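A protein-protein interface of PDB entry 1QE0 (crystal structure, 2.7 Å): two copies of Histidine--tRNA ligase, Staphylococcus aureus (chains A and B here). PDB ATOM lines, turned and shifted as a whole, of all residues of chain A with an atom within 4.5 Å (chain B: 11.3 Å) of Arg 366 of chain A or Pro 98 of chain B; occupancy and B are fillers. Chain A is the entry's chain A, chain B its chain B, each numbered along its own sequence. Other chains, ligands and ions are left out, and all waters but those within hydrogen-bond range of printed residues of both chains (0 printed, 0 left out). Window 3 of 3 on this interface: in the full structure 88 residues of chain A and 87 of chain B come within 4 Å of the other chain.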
ATOM      1  N   ASP A 362      15.748  26.607 -25.647  1.00  0.00           N
ATOM      2  CA  ASP A 362      14.797  25.555 -25.312  1.00  0.00           C
ATOM      3  C   ASP A 362      13.517  25.523 -26.131  1.00  0.00           C
ATOM      4  O   ASP A 362      12.672  26.420 -26.054  1.00  0.00           O
ATOM      5  CB  ASP A 362      14.451  25.612 -23.832  1.00  0.00           C
ATOM      6  CG  ASP A 362      13.383  24.621 -23.450  1.00  0.00           C
ATOM      7  OD1 ASP A 362      12.305  25.094 -23.026  1.00  0.00           O
ATOM      8  OD2 ASP A 362      13.622  23.386 -23.586  1.00  0.00           O
ATOM      9  N   LEU A 364      10.388  22.721 -27.030  1.00  0.00           N
ATOM     10  CA  LEU A 364       9.755  21.951 -25.910  1.00  0.00           C
ATOM     11  C   LEU A 364       9.144  22.730 -24.691  1.00  0.00           C
ATOM     12  O   LEU A 364       8.559  22.115 -23.800  1.00  0.00           O
ATOM     13  CB  LEU A 364      10.747  20.901 -25.341  1.00  0.00           C
ATOM     14  CG  LEU A 364      10.646  19.397 -25.627  1.00  0.00           C
ATOM     15  CD1 LEU A 364      10.887  19.059 -27.075  1.00  0.00           C
ATOM     16  CD2 LEU A 364      11.665  18.709 -24.801  1.00  0.00           C
ATOM     17  N   GLN A 365       9.321  24.048 -24.635  1.00  0.00           N
ATOM     18  CA  GLN A 365       8.777  24.882 -23.559  1.00  0.00           C
ATOM     19  C   GLN A 365       8.713  24.251 -22.174  1.00  0.00           C
ATOM     20  O   GLN A 365       7.662  23.740 -21.784  1.00  0.00           O
ATOM     21  CB  GLN A 365       7.364  25.340 -23.914  1.00  0.00           C
ATOM     22  CG  GLN A 365       7.270  26.288 -25.080  1.00  0.00           C
ATOM     23  CD  GLN A 365       5.850  26.399 -25.606  1.00  0.00           C
ATOM     24  OE1 GLN A 365       5.453  27.434 -26.134  1.00  0.00           O
ATOM     25  NE2 GLN A 365       5.077  25.335 -25.467  1.00  0.00           N
ATOM     26  N   ARG A 366       9.814  24.287 -21.422  1.00  0.00           N
ATOM     27  CA  ARG A 366       9.814  23.727 -20.069  1.00  0.00           C
ATOM     28  C   ARG A 366      10.123  24.718 -18.971  1.00  0.00           C
ATOM     29  O   ARG A 366      10.418  25.873 -19.231  1.00  0.00           O
ATOM     30  CB  ARG A 366      10.708  22.486 -19.951  1.00  0.00           C
ATOM     31  CG  ARG A 366      11.980  22.507 -20.720  1.00  0.00           C
ATOM     32  CD  ARG A 366      12.438  21.081 -21.070  1.00  0.00           C
ATOM     33  NE  ARG A 366      13.534  21.113 -22.035  1.00  0.00           N
ATOM     34  CZ  ARG A 366      14.082  20.064 -22.644  1.00  0.00           C
ATOM     35  NH1 ARG A 366      15.063  20.276 -23.505  1.00  0.00           N
ATOM     36  NH2 ARG A 366      13.706  18.821 -22.381  1.00  0.00           N
ATOM     37  N   LYS A 367      10.001  24.264 -17.730  1.00  0.00           N
ATOM     38  CA  LYS A 367      10.267  25.089 -16.543  1.00  0.00           C
ATOM     39  C   LYS A 367      11.768  25.329 -16.434  1.00  0.00           C
ATOM     40  O   LYS A 367      12.550  24.493 -16.880  1.00  0.00           O
ATOM     41  CB  LYS A 367       9.825  24.330 -15.284  1.00  0.00           C
ATOM     42  CG  LYS A 367       8.641  23.423 -15.497  1.00  0.00           C
ATOM     43  CD  LYS A 367       8.559  22.346 -14.415  1.00  0.00           C
ATOM     44  CE  LYS A 367       8.098  22.882 -13.052  1.00  0.00           C
ATOM     45  NZ  LYS A 367       6.612  23.156 -12.964  1.00  0.00           N
ATOM     46  N   ILE A 368      12.176  26.393 -15.748  1.00  0.00           N
ATOM     47  CA  ILE A 368      13.601  26.698 -15.566  1.00  0.00           C
ATOM     48  C   ILE A 368      14.394  25.459 -15.140  1.00  0.00           C
ATOM     49  O   ILE A 368      15.452  25.204 -15.683  1.00  0.00           O
ATOM     50  CB  ILE A 368      13.891  27.741 -14.432  1.00  0.00           C
ATOM     51  CG1 ILE A 368      13.065  29.001 -14.564  1.00  0.00           C
ATOM     52  CG2 ILE A 368      15.360  28.189 -14.447  1.00  0.00           C
ATOM     53  CD1 ILE A 368      13.482  30.022 -13.502  1.00  0.00           C
ATOM     54  N   GLY A 370      14.008  22.539 -15.826  1.00  0.00           N
ATOM     55  CA  GLY A 370      14.102  21.724 -17.032  1.00  0.00           C
ATOM     56  C   GLY A 370      14.978  22.313 -18.110  1.00  0.00           C
ATOM     57  O   GLY A 370      15.614  21.595 -18.899  1.00  0.00           O
ATOM     58  N   GLN A 371      14.960  23.632 -18.204  1.00  0.00           N
ATOM     59  CA  GLN A 371      15.812  24.284 -19.163  1.00  0.00           C
ATOM     60  C   GLN A 371      17.243  24.188 -18.646  1.00  0.00           C
ATOM     61  O   GLN A 371      18.135  23.769 -19.384  1.00  0.00           O
ATOM     62  CB  GLN A 371      15.374  25.721 -19.370  1.00  0.00           C
ATOM     63  CG  GLN A 371      14.198  25.822 -20.336  1.00  0.00           C
ATOM     64  CD  GLN A 371      13.776  27.222 -20.532  1.00  0.00           C
ATOM     65  OE1 GLN A 371      14.585  28.054 -20.893  1.00  0.00           O
ATOM     66  NE2 GLN A 371      12.539  27.528 -20.204  1.00  0.00           N
ATOM     67  N   GLN A 374      18.695  20.880 -19.237  1.00  0.00           N
ATOM     68  CA  GLN A 374      19.026  20.700 -20.640  1.00  0.00           C
ATOM     69  C   GLN A 374      20.353  21.371 -20.898  1.00  0.00           C
ATOM     70  O   GLN A 374      21.256  20.782 -21.524  1.00  0.00           O
ATOM     71  CB  GLN A 374      17.913  21.267 -21.515  1.00  0.00           C
ATOM     72  CG  GLN A 374      18.136  21.188 -23.034  1.00  0.00           C
ATOM     73  CD  GLN A 374      18.224  19.783 -23.640  1.00  0.00           C
ATOM     74  OE1 GLN A 374      17.961  18.764 -22.999  1.00  0.00           O
ATOM     75  NE2 GLN A 374      18.616  19.741 -24.898  1.00  0.00           N
ATOM     76  N   ARG A 377      22.763  19.080 -19.676  1.00  0.00           N
ATOM     77  CA  ARG A 377      22.802  17.885 -20.495  1.00  0.00           C
ATOM     78  C   ARG A 377      23.630  18.147 -21.775  1.00  0.00           C
ATOM     79  O   ARG A 377      24.468  17.337 -22.172  1.00  0.00           O
ATOM     80  CB  ARG A 377      21.361  17.451 -20.803  1.00  0.00           C
ATOM     81  CG  ARG A 377      21.203  16.279 -21.757  1.00  0.00           C
ATOM     82  CD  ARG A 377      19.885  15.565 -21.552  1.00  0.00           C
ATOM     83  NE  ARG A 377      18.730  16.466 -21.512  1.00  0.00           N
ATOM     84  CZ  ARG A 377      18.165  16.913 -20.389  1.00  0.00           C
ATOM     85  NH1 ARG A 377      17.113  17.719 -20.438  1.00  0.00           N
ATOM     86  NH2 ARG A 377      18.658  16.569 -19.206  1.00  0.00           N
ATOM     87  N   ASN B  34      24.227  22.940 -32.993  1.00  0.00           N
ATOM     88  CA  ASN B  34      24.098  21.824 -32.090  1.00  0.00           C
ATOM     89  C   ASN B  34      23.495  20.576 -32.684  1.00  0.00           C
ATOM     90  O   ASN B  34      22.748  19.870 -31.989  1.00  0.00           O
ATOM     91  CB  ASN B  34      23.322  22.232 -30.843  1.00  0.00           C
ATOM     92  CG  ASN B  34      23.572  21.308 -29.682  1.00  0.00           C
ATOM     93  OD1 ASN B  34      24.646  20.716 -29.586  1.00  0.00           O
ATOM     94  ND2 ASN B  34      22.570  21.136 -28.808  1.00  0.00           N
ATOM     95  N   TYR B  89      17.006   6.034 -35.205  1.00  0.00           N
ATOM     96  CA  TYR B  89      16.292   6.749 -34.172  1.00  0.00           C
ATOM     97  C   TYR B  89      15.373   5.774 -33.457  1.00  0.00           C
ATOM     98  O   TYR B  89      15.346   5.743 -32.229  1.00  0.00           O
ATOM     99  CB  TYR B  89      15.490   7.875 -34.816  1.00  0.00           C
ATOM    100  CG  TYR B  89      14.498   8.547 -33.895  1.00  0.00           C
ATOM    101  CD1 TYR B  89      14.837   9.705 -33.204  1.00  0.00           C
ATOM    102  CD2 TYR B  89      13.198   8.049 -33.754  1.00  0.00           C
ATOM    103  CE1 TYR B  89      13.910  10.355 -32.406  1.00  0.00           C
ATOM    104  CE2 TYR B  89      12.262   8.694 -32.957  1.00  0.00           C
ATOM    105  CZ  TYR B  89      12.623   9.845 -32.290  1.00  0.00           C
ATOM    106  OH  TYR B  89      11.682  10.504 -31.530  1.00  0.00           O
ATOM    107  N   HIS B  92      17.349   2.750 -31.700  1.00  0.00           N
ATOM    108  CA  HIS B  92      18.089   3.175 -30.507  1.00  0.00           C
ATOM    109  C   HIS B  92      17.200   3.835 -29.455  1.00  0.00           C
ATOM    110  O   HIS B  92      17.684   4.458 -28.512  1.00  0.00           O
ATOM    111  CB  HIS B  92      19.242   4.100 -30.906  1.00  0.00           C
ATOM    112  CG  HIS B  92      20.255   3.420 -31.769  1.00  0.00           C
ATOM    113  ND1 HIS B  92      20.325   3.619 -33.130  1.00  0.00           N
ATOM    114  CD2 HIS B  92      21.144   2.436 -31.486  1.00  0.00           C
ATOM    115  CE1 HIS B  92      21.202   2.780 -33.648  1.00  0.00           C
ATOM    116  NE2 HIS B  92      21.712   2.051 -32.673  1.00  0.00           N
ATOM    117  N   LYS B  93      15.893   3.732 -29.664  1.00  0.00           N
ATOM    118  CA  LYS B  93      14.909   4.289 -28.758  1.00  0.00           C
ATOM    119  C   LYS B  93      15.288   5.689 -28.314  1.00  0.00           C
ATOM    120  O   LYS B  93      15.325   6.002 -27.120  1.00  0.00           O
ATOM    121  CB  LYS B  93      14.728   3.344 -27.571  1.00  0.00           C
ATOM    122  CG  LYS B  93      14.171   1.970 -27.986  1.00  0.00           C
ATOM    123  CD  LYS B  93      14.403   0.892 -26.913  1.00  0.00           C
ATOM    124  CE  LYS B  93      13.407  -0.261 -27.049  1.00  0.00           C
ATOM    125  NZ  LYS B  93      13.450  -0.947 -28.379  1.00  0.00           N
ATOM    126  N   MET B  94      15.480   6.553 -29.301  1.00  0.00           N
ATOM    127  CA  MET B  94      15.866   7.951 -29.071  1.00  0.00           C
ATOM    128  C   MET B  94      14.727   8.821 -28.564  1.00  0.00           C
ATOM    129  O   MET B  94      14.946   9.855 -27.952  1.00  0.00           O
ATOM    130  CB  MET B  94      16.444   8.555 -30.349  1.00  0.00           C
ATOM    131  CG  MET B  94      17.675   7.831 -30.838  1.00  0.00           C
ATOM    132  SD  MET B  94      18.528   8.764 -32.052  1.00  0.00           S
ATOM    133  CE  MET B  94      19.698   7.545 -32.624  1.00  0.00           C
ATOM    134  N   GLN B  95      13.505   8.402 -28.862  1.00  0.00           N
ATOM    135  CA  GLN B  95      12.306   9.103 -28.419  1.00  0.00           C
ATOM    136  C   GLN B  95      12.339   9.225 -26.904  1.00  0.00           C
ATOM    137  O   GLN B  95      11.806  10.166 -26.353  1.00  0.00           O
ATOM    138  CB  GLN B  95      11.050   8.338 -28.853  1.00  0.00           C
ATOM    139  CG  GLN B  95      11.005   6.853 -28.437  1.00  0.00           C
ATOM    140  CD  GLN B  95      11.811   5.883 -29.341  1.00  0.00           C
ATOM    141  OE1 GLN B  95      12.616   6.272 -30.159  1.00  0.00           O
ATOM    142  NE2 GLN B  95      11.582   4.605 -29.159  1.00  0.00           N
ATOM    143  N   GLY B  96      13.026   8.287 -26.249  1.00  0.00           N
ATOM    144  CA  GLY B  96      13.121   8.279 -24.798  1.00  0.00           C
ATOM    145  C   GLY B  96      14.300   9.060 -24.269  1.00  0.00           C
ATOM    146  O   GLY B  96      14.549   9.085 -23.057  1.00  0.00           O
ATOM    147  N   ASN B  97      15.056   9.666 -25.169  1.00  0.00           N
ATOM    148  CA  ASN B  97      16.203  10.457 -24.781  1.00  0.00           C
ATOM    149  C   ASN B  97      15.819  11.680 -23.967  1.00  0.00           C
ATOM    150  O   ASN B  97      14.912  12.436 -24.331  1.00  0.00           O
ATOM    151  CB  ASN B  97      16.907  10.935 -26.015  1.00  0.00           C
ATOM    152  CG  ASN B  97      18.256  10.382 -26.123  1.00  0.00           C
ATOM    153  OD1 ASN B  97      18.473   9.398 -26.821  1.00  0.00           O
ATOM    154  ND2 ASN B  97      19.198  10.983 -25.397  1.00  0.00           N
ATOM    155  N   PRO B  98      16.553  11.939 -22.886  1.00  0.00           N
ATOM    156  CA  PRO B  98      16.242  13.105 -22.055  1.00  0.00           C
ATOM    157  C   PRO B  98      16.449  14.430 -22.823  1.00  0.00           C
ATOM    158  O   PRO B  98      15.789  15.426 -22.561  1.00  0.00           O
ATOM    159  CB  PRO B  98      17.203  12.932 -20.882  1.00  0.00           C
ATOM    160  CG  PRO B  98      18.395  12.283 -21.532  1.00  0.00           C
ATOM    161  CD  PRO B  98      17.736  11.227 -22.379  1.00  0.00           C
ATOM    162  N   ASN B  99      17.368  14.413 -23.785  1.00  0.00           N
ATOM    163  CA  ASN B  99      17.680  15.579 -24.624  1.00  0.00           C
ATOM    164  C   ASN B  99      16.858  15.568 -25.914  1.00  0.00           C
ATOM    165  O   ASN B  99      17.076  14.729 -26.795  1.00  0.00           O
ATOM    166  CB  ASN B  99      19.171  15.567 -24.964  1.00  0.00           C
ATOM    167  CG  ASN B  99      19.527  16.501 -26.099  1.00  0.00           C
ATOM    168  OD1 ASN B  99      18.733  17.342 -26.500  1.00  0.00           O
ATOM    169  ND2 ASN B  99      20.744  16.370 -26.611  1.00  0.00           N
ATOM    170  N   GLN B 100      15.934  16.515 -26.020  1.00  0.00           N
ATOM    171  CA  GLN B 100      15.066  16.641 -27.196  1.00  0.00           C
ATOM    172  C   GLN B 100      14.936  18.128 -27.591  1.00  0.00           C
ATOM    173  O   GLN B 100      15.080  19.007 -26.736  1.00  0.00           O
ATOM    174  CB  GLN B 100      13.674  16.049 -26.920  1.00  0.00           C
ATOM    175  CG  GLN B 100      13.653  14.581 -26.485  1.00  0.00           C
ATOM    176  CD  GLN B 100      13.713  13.592 -27.629  1.00  0.00           C
ATOM    177  OE1 GLN B 100      13.081  13.776 -28.700  1.00  0.00           O
ATOM    178  NE2 GLN B 100      14.451  12.505 -27.406  1.00  0.00           N
ATOM    179  N   PRO B 101      14.671  18.433 -28.881  1.00  0.00           N
ATOM    180  CA  PRO B 101      14.504  17.479 -29.990  1.00  0.00           C
ATOM    181  C   PRO B 101      15.805  16.814 -30.390  1.00  0.00           C
ATOM    182  O   PRO B 101      16.903  17.318 -30.101  1.00  0.00           O
ATOM    183  CB  PRO B 101      13.982  18.363 -31.141  1.00  0.00           C
ATOM    184  CG  PRO B 101      14.614  19.665 -30.884  1.00  0.00           C
ATOM    185  CD  PRO B 101      14.531  19.820 -29.365  1.00  0.00           C
ATOM    186  N   ILE B 102      15.689  15.643 -30.985  1.00  0.00           N
ATOM    187  CA  ILE B 102      16.864  14.965 -31.460  1.00  0.00           C
ATOM    188  C   ILE B 102      17.297  15.747 -32.692  1.00  0.00           C
ATOM    189  O   ILE B 102      16.554  15.850 -33.657  1.00  0.00           O
ATOM    190  CB  ILE B 102      16.527  13.507 -31.793  1.00  0.00           C
ATOM    191  CG1 ILE B 102      16.189  12.768 -30.503  1.00  0.00           C
ATOM    192  CG2 ILE B 102      17.648  12.833 -32.511  1.00  0.00           C
ATOM    193  CD1 ILE B 102      17.173  13.011 -29.386  1.00  0.00           C
ATOM    194  N   LYS B 103      18.455  16.390 -32.596  1.00  0.00           N
ATOM    195  CA  LYS B 103      19.021  17.173 -33.703  1.00  0.00           C
ATOM    196  C   LYS B 103      20.218  16.415 -34.266  1.00  0.00           C
ATOM    197  O   LYS B 103      21.298  16.482 -33.696  1.00  0.00           O
ATOM    198  CB  LYS B 103      19.464  18.567 -33.210  1.00  0.00           C
ATOM    199  CG  LYS B 103      18.291  19.468 -32.843  1.00  0.00           C
ATOM    200  CD  LYS B 103      18.687  20.639 -31.971  1.00  0.00           C
ATOM    201  CE  LYS B 103      19.027  21.873 -32.773  1.00  0.00           C
ATOM    202  NZ  LYS B 103      19.183  23.077 -31.927  1.00  0.00           N
ATOM    203  N   ILE B 132      14.062  15.895 -34.816  1.00  0.00           N
ATOM    204  CA  ILE B 132      12.874  15.137 -34.490  1.00  0.00           C
ATOM    205  C   ILE B 132      12.429  15.268 -33.041  1.00  0.00           C
ATOM    206  O   ILE B 132      13.244  15.226 -32.118  1.00  0.00           O
ATOM    207  CB  ILE B 132      13.056  13.649 -34.856  1.00  0.00           C
ATOM    208  CG1 ILE B 132      13.907  13.521 -36.128  1.00  0.00           C
ATOM    209  CG2 ILE B 132      11.667  12.992 -35.106  1.00  0.00           C
ATOM    210  CD1 ILE B 132      14.260  12.107 -36.488  1.00  0.00           C
ATOM    211  N   GLY B 133      11.124  15.478 -32.864  1.00  0.00           N
ATOM    212  CA  GLY B 133      10.547  15.592 -31.536  1.00  0.00           C
ATOM    213  C   GLY B 133      10.232  16.964 -30.956  1.00  0.00           C
ATOM    214  O   GLY B 133      10.369  17.150 -29.755  1.00  0.00           O
ATOM    215  N   ALA B 134       9.828  17.931 -31.767  1.00  0.00           N
ATOM    216  CA  ALA B 134       9.488  19.246 -31.227  1.00  0.00           C
ATOM    217  C   ALA B 134       8.832  20.095 -32.304  1.00  0.00           C
ATOM    218  O   ALA B 134       9.481  20.941 -32.919  1.00  0.00           O
ATOM    219  CB  ALA B 134      10.730  19.957 -30.671  1.00  0.00           C
ATOM    220  N   ASN B 136       7.472  22.924 -33.630  1.00  0.00           N
ATOM    221  CA  ASN B 136       7.480  24.259 -33.086  1.00  0.00           C
ATOM    222  C   ASN B 136       8.008  25.235 -34.119  1.00  0.00           C
ATOM    223  O   ASN B 136       9.031  24.991 -34.743  1.00  0.00           O
ATOM    224  CB  ASN B 136       8.354  24.222 -31.815  1.00  0.00           C
ATOM    225  CG  ASN B 136       8.561  25.569 -31.179  1.00  0.00           C
ATOM    226  OD1 ASN B 136       8.312  26.610 -31.771  1.00  0.00           O
ATOM    227  ND2 ASN B 136       9.068  25.555 -29.961  1.00  0.00           N
ATOM    228  N   SER B 138       9.536  27.990 -33.940  1.00  0.00           N
ATOM    229  CA  SER B 138      10.909  28.430 -33.671  1.00  0.00           C
ATOM    230  C   SER B 138      11.955  27.442 -34.139  1.00  0.00           C
ATOM    231  O   SER B 138      13.082  27.844 -34.401  1.00  0.00           O
ATOM    232  CB  SER B 138      11.134  28.709 -32.205  1.00  0.00           C
ATOM    233  OG  SER B 138      11.202  27.504 -31.477  1.00  0.00           O
ATOM    234  N   VAL B 139      11.588  26.160 -34.212  1.00  0.00           N
ATOM    235  CA  VAL B 139      12.486  25.091 -34.685  1.00  0.00           C
ATOM    236  C   VAL B 139      12.568  25.144 -36.216  1.00  0.00           C
ATOM    237  O   VAL B 139      13.647  24.995 -36.785  1.00  0.00           O
ATOM    238  CB  VAL B 139      11.994  23.671 -34.268  1.00  0.00           C
ATOM    239  CG1 VAL B 139      12.863  22.605 -34.904  1.00  0.00           C
ATOM    240  CG2 VAL B 139      12.030  23.536 -32.755  1.00  0.00           C
ATOM    241  N   GLU B 301       6.289  10.849 -33.342  1.00  0.00           N
ATOM    242  CA  GLU B 301       7.109  12.049 -33.335  1.00  0.00           C
ATOM    243  C   GLU B 301       6.984  12.900 -34.591  1.00  0.00           C
ATOM    244  O   GLU B 301       6.761  12.391 -35.702  1.00  0.00           O
ATOM    245  CB  GLU B 301       8.571  11.670 -33.129  1.00  0.00           C
ATOM    246  CG  GLU B 301       8.819  10.950 -31.839  1.00  0.00           C
ATOM    247  CD  GLU B 301       8.376  11.768 -30.643  1.00  0.00           C
ATOM    248  OE1 GLU B 301       8.223  13.007 -30.786  1.00  0.00           O
ATOM    249  OE2 GLU B 301       8.176  11.176 -29.553  1.00  0.00           O
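The backbone carbonyl oxygen of Gln 100 of chain B is in hydrogen-bond range of the guanidinium group of Arg 366 of chain A (3.5 Å). The side-chain amide nitrogen of Gln 374 of chain A lies within hydrogen-bond range of the side-chain amide oxygen of Asn 99 of chain B. The guanidinium group of Arg 377 of chain A sits at hydrogen-bond distance from the backbone carbonyl oxygen of Pro 98 of chain B, 3.3 Å away. The guanidinium group (NE) of Arg 377 of chain A lies close to the backbone NH (N) of Asn 99 of chain B (3.4 Å).
NE of Arg 366 of chain A is in salt-bridge range of OD2 of Asp 362 of chain A (2.8 Å). NE2 of Gln 371 of chain A sits at hydrogen-bond distance from O of Arg 366 of chain A. NH1 of Arg 366 of chain A lies close to OE1 of Gln 374 of chain A. The guanidinium group (NE) of Arg 377 of chain A sits at hydrogen-bond distance from the side-chain amide oxygen (OE1) of Gln 374 of chain A (2.8 Å). The side-chain amide nitrogen of Gln 100 of chain B is in hydrogen-bond range of the backbone carbonyl oxygen of Met 94 of chain B, at 2.8 Å. O of Asn 97 of chain B is in hydrogen-bond range of NE2 of Gln 100 of chain B.
Leu 364 of chain A touches Gln 100 of chain B (CD2 to O, 3.9 Å). Leu 364 of chain A touches Gly 133 of chain B. Ala 134 of chain B touches Leu 364 of chain A. NH2 of Arg 366 of chain A touches O of Pro 98 of chain B, 3.99 Å away.
No residue of chain B comes within 4 Å of Asp 362 of chain A. No residue of chain B comes within 4 Å of Gln 365 of chain A. Of the printed residues of chain B, Arg 366 of chain A touches Pro 98 and Gln 100. No residue of chain B comes within 4 Å of Lys 367 of chain A. No residue of chain B comes within 4 Å of Gly 370 of chain A. No residue of chain B comes within 4 Å of Gln 371 of chain A. Printed residues of chain B within 4 Å of Gln 374 of chain A: Asn 99. Printed residues of chain B within 4 Å of Arg 377 of chain A: Pro 98 and Asn 99. Asn 97 of chain B touches none of the printed residues of chain A. Of the printed residues of chain A, Pro 98 of chain B touches Arg 366 and Arg 377. Printed residues of chain A within 4 Å of Gln 100 of chain B: Leu 364 and Arg 366. Of the printed residues of chain A, Ala 134 of chain B touches Leu 364. The nearest printed residue of chain B that does not touch Arg 366 of chain A is Asn 99 of chain B (5.5 Å).
Hydrophobic or aromatic side chains of chain B that line the printed part of chain A: Pro 98 and Ala 134. Printed residues of chain A that touch a printed residue of chain B: Leu 364, Arg 366, Gln 374 and Arg 377. Among the printed residues, 8 pairs touch across the chains. Among the printed residues, no Asp or Glu carboxylate lies within 4 Å of a Lys or Arg side-chain nitrogen of the other chain.
No position is printed for both chains. Of the 8 pairs that touch across the chains among the printed residues, none has its exchanged pair printed and touching as well.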
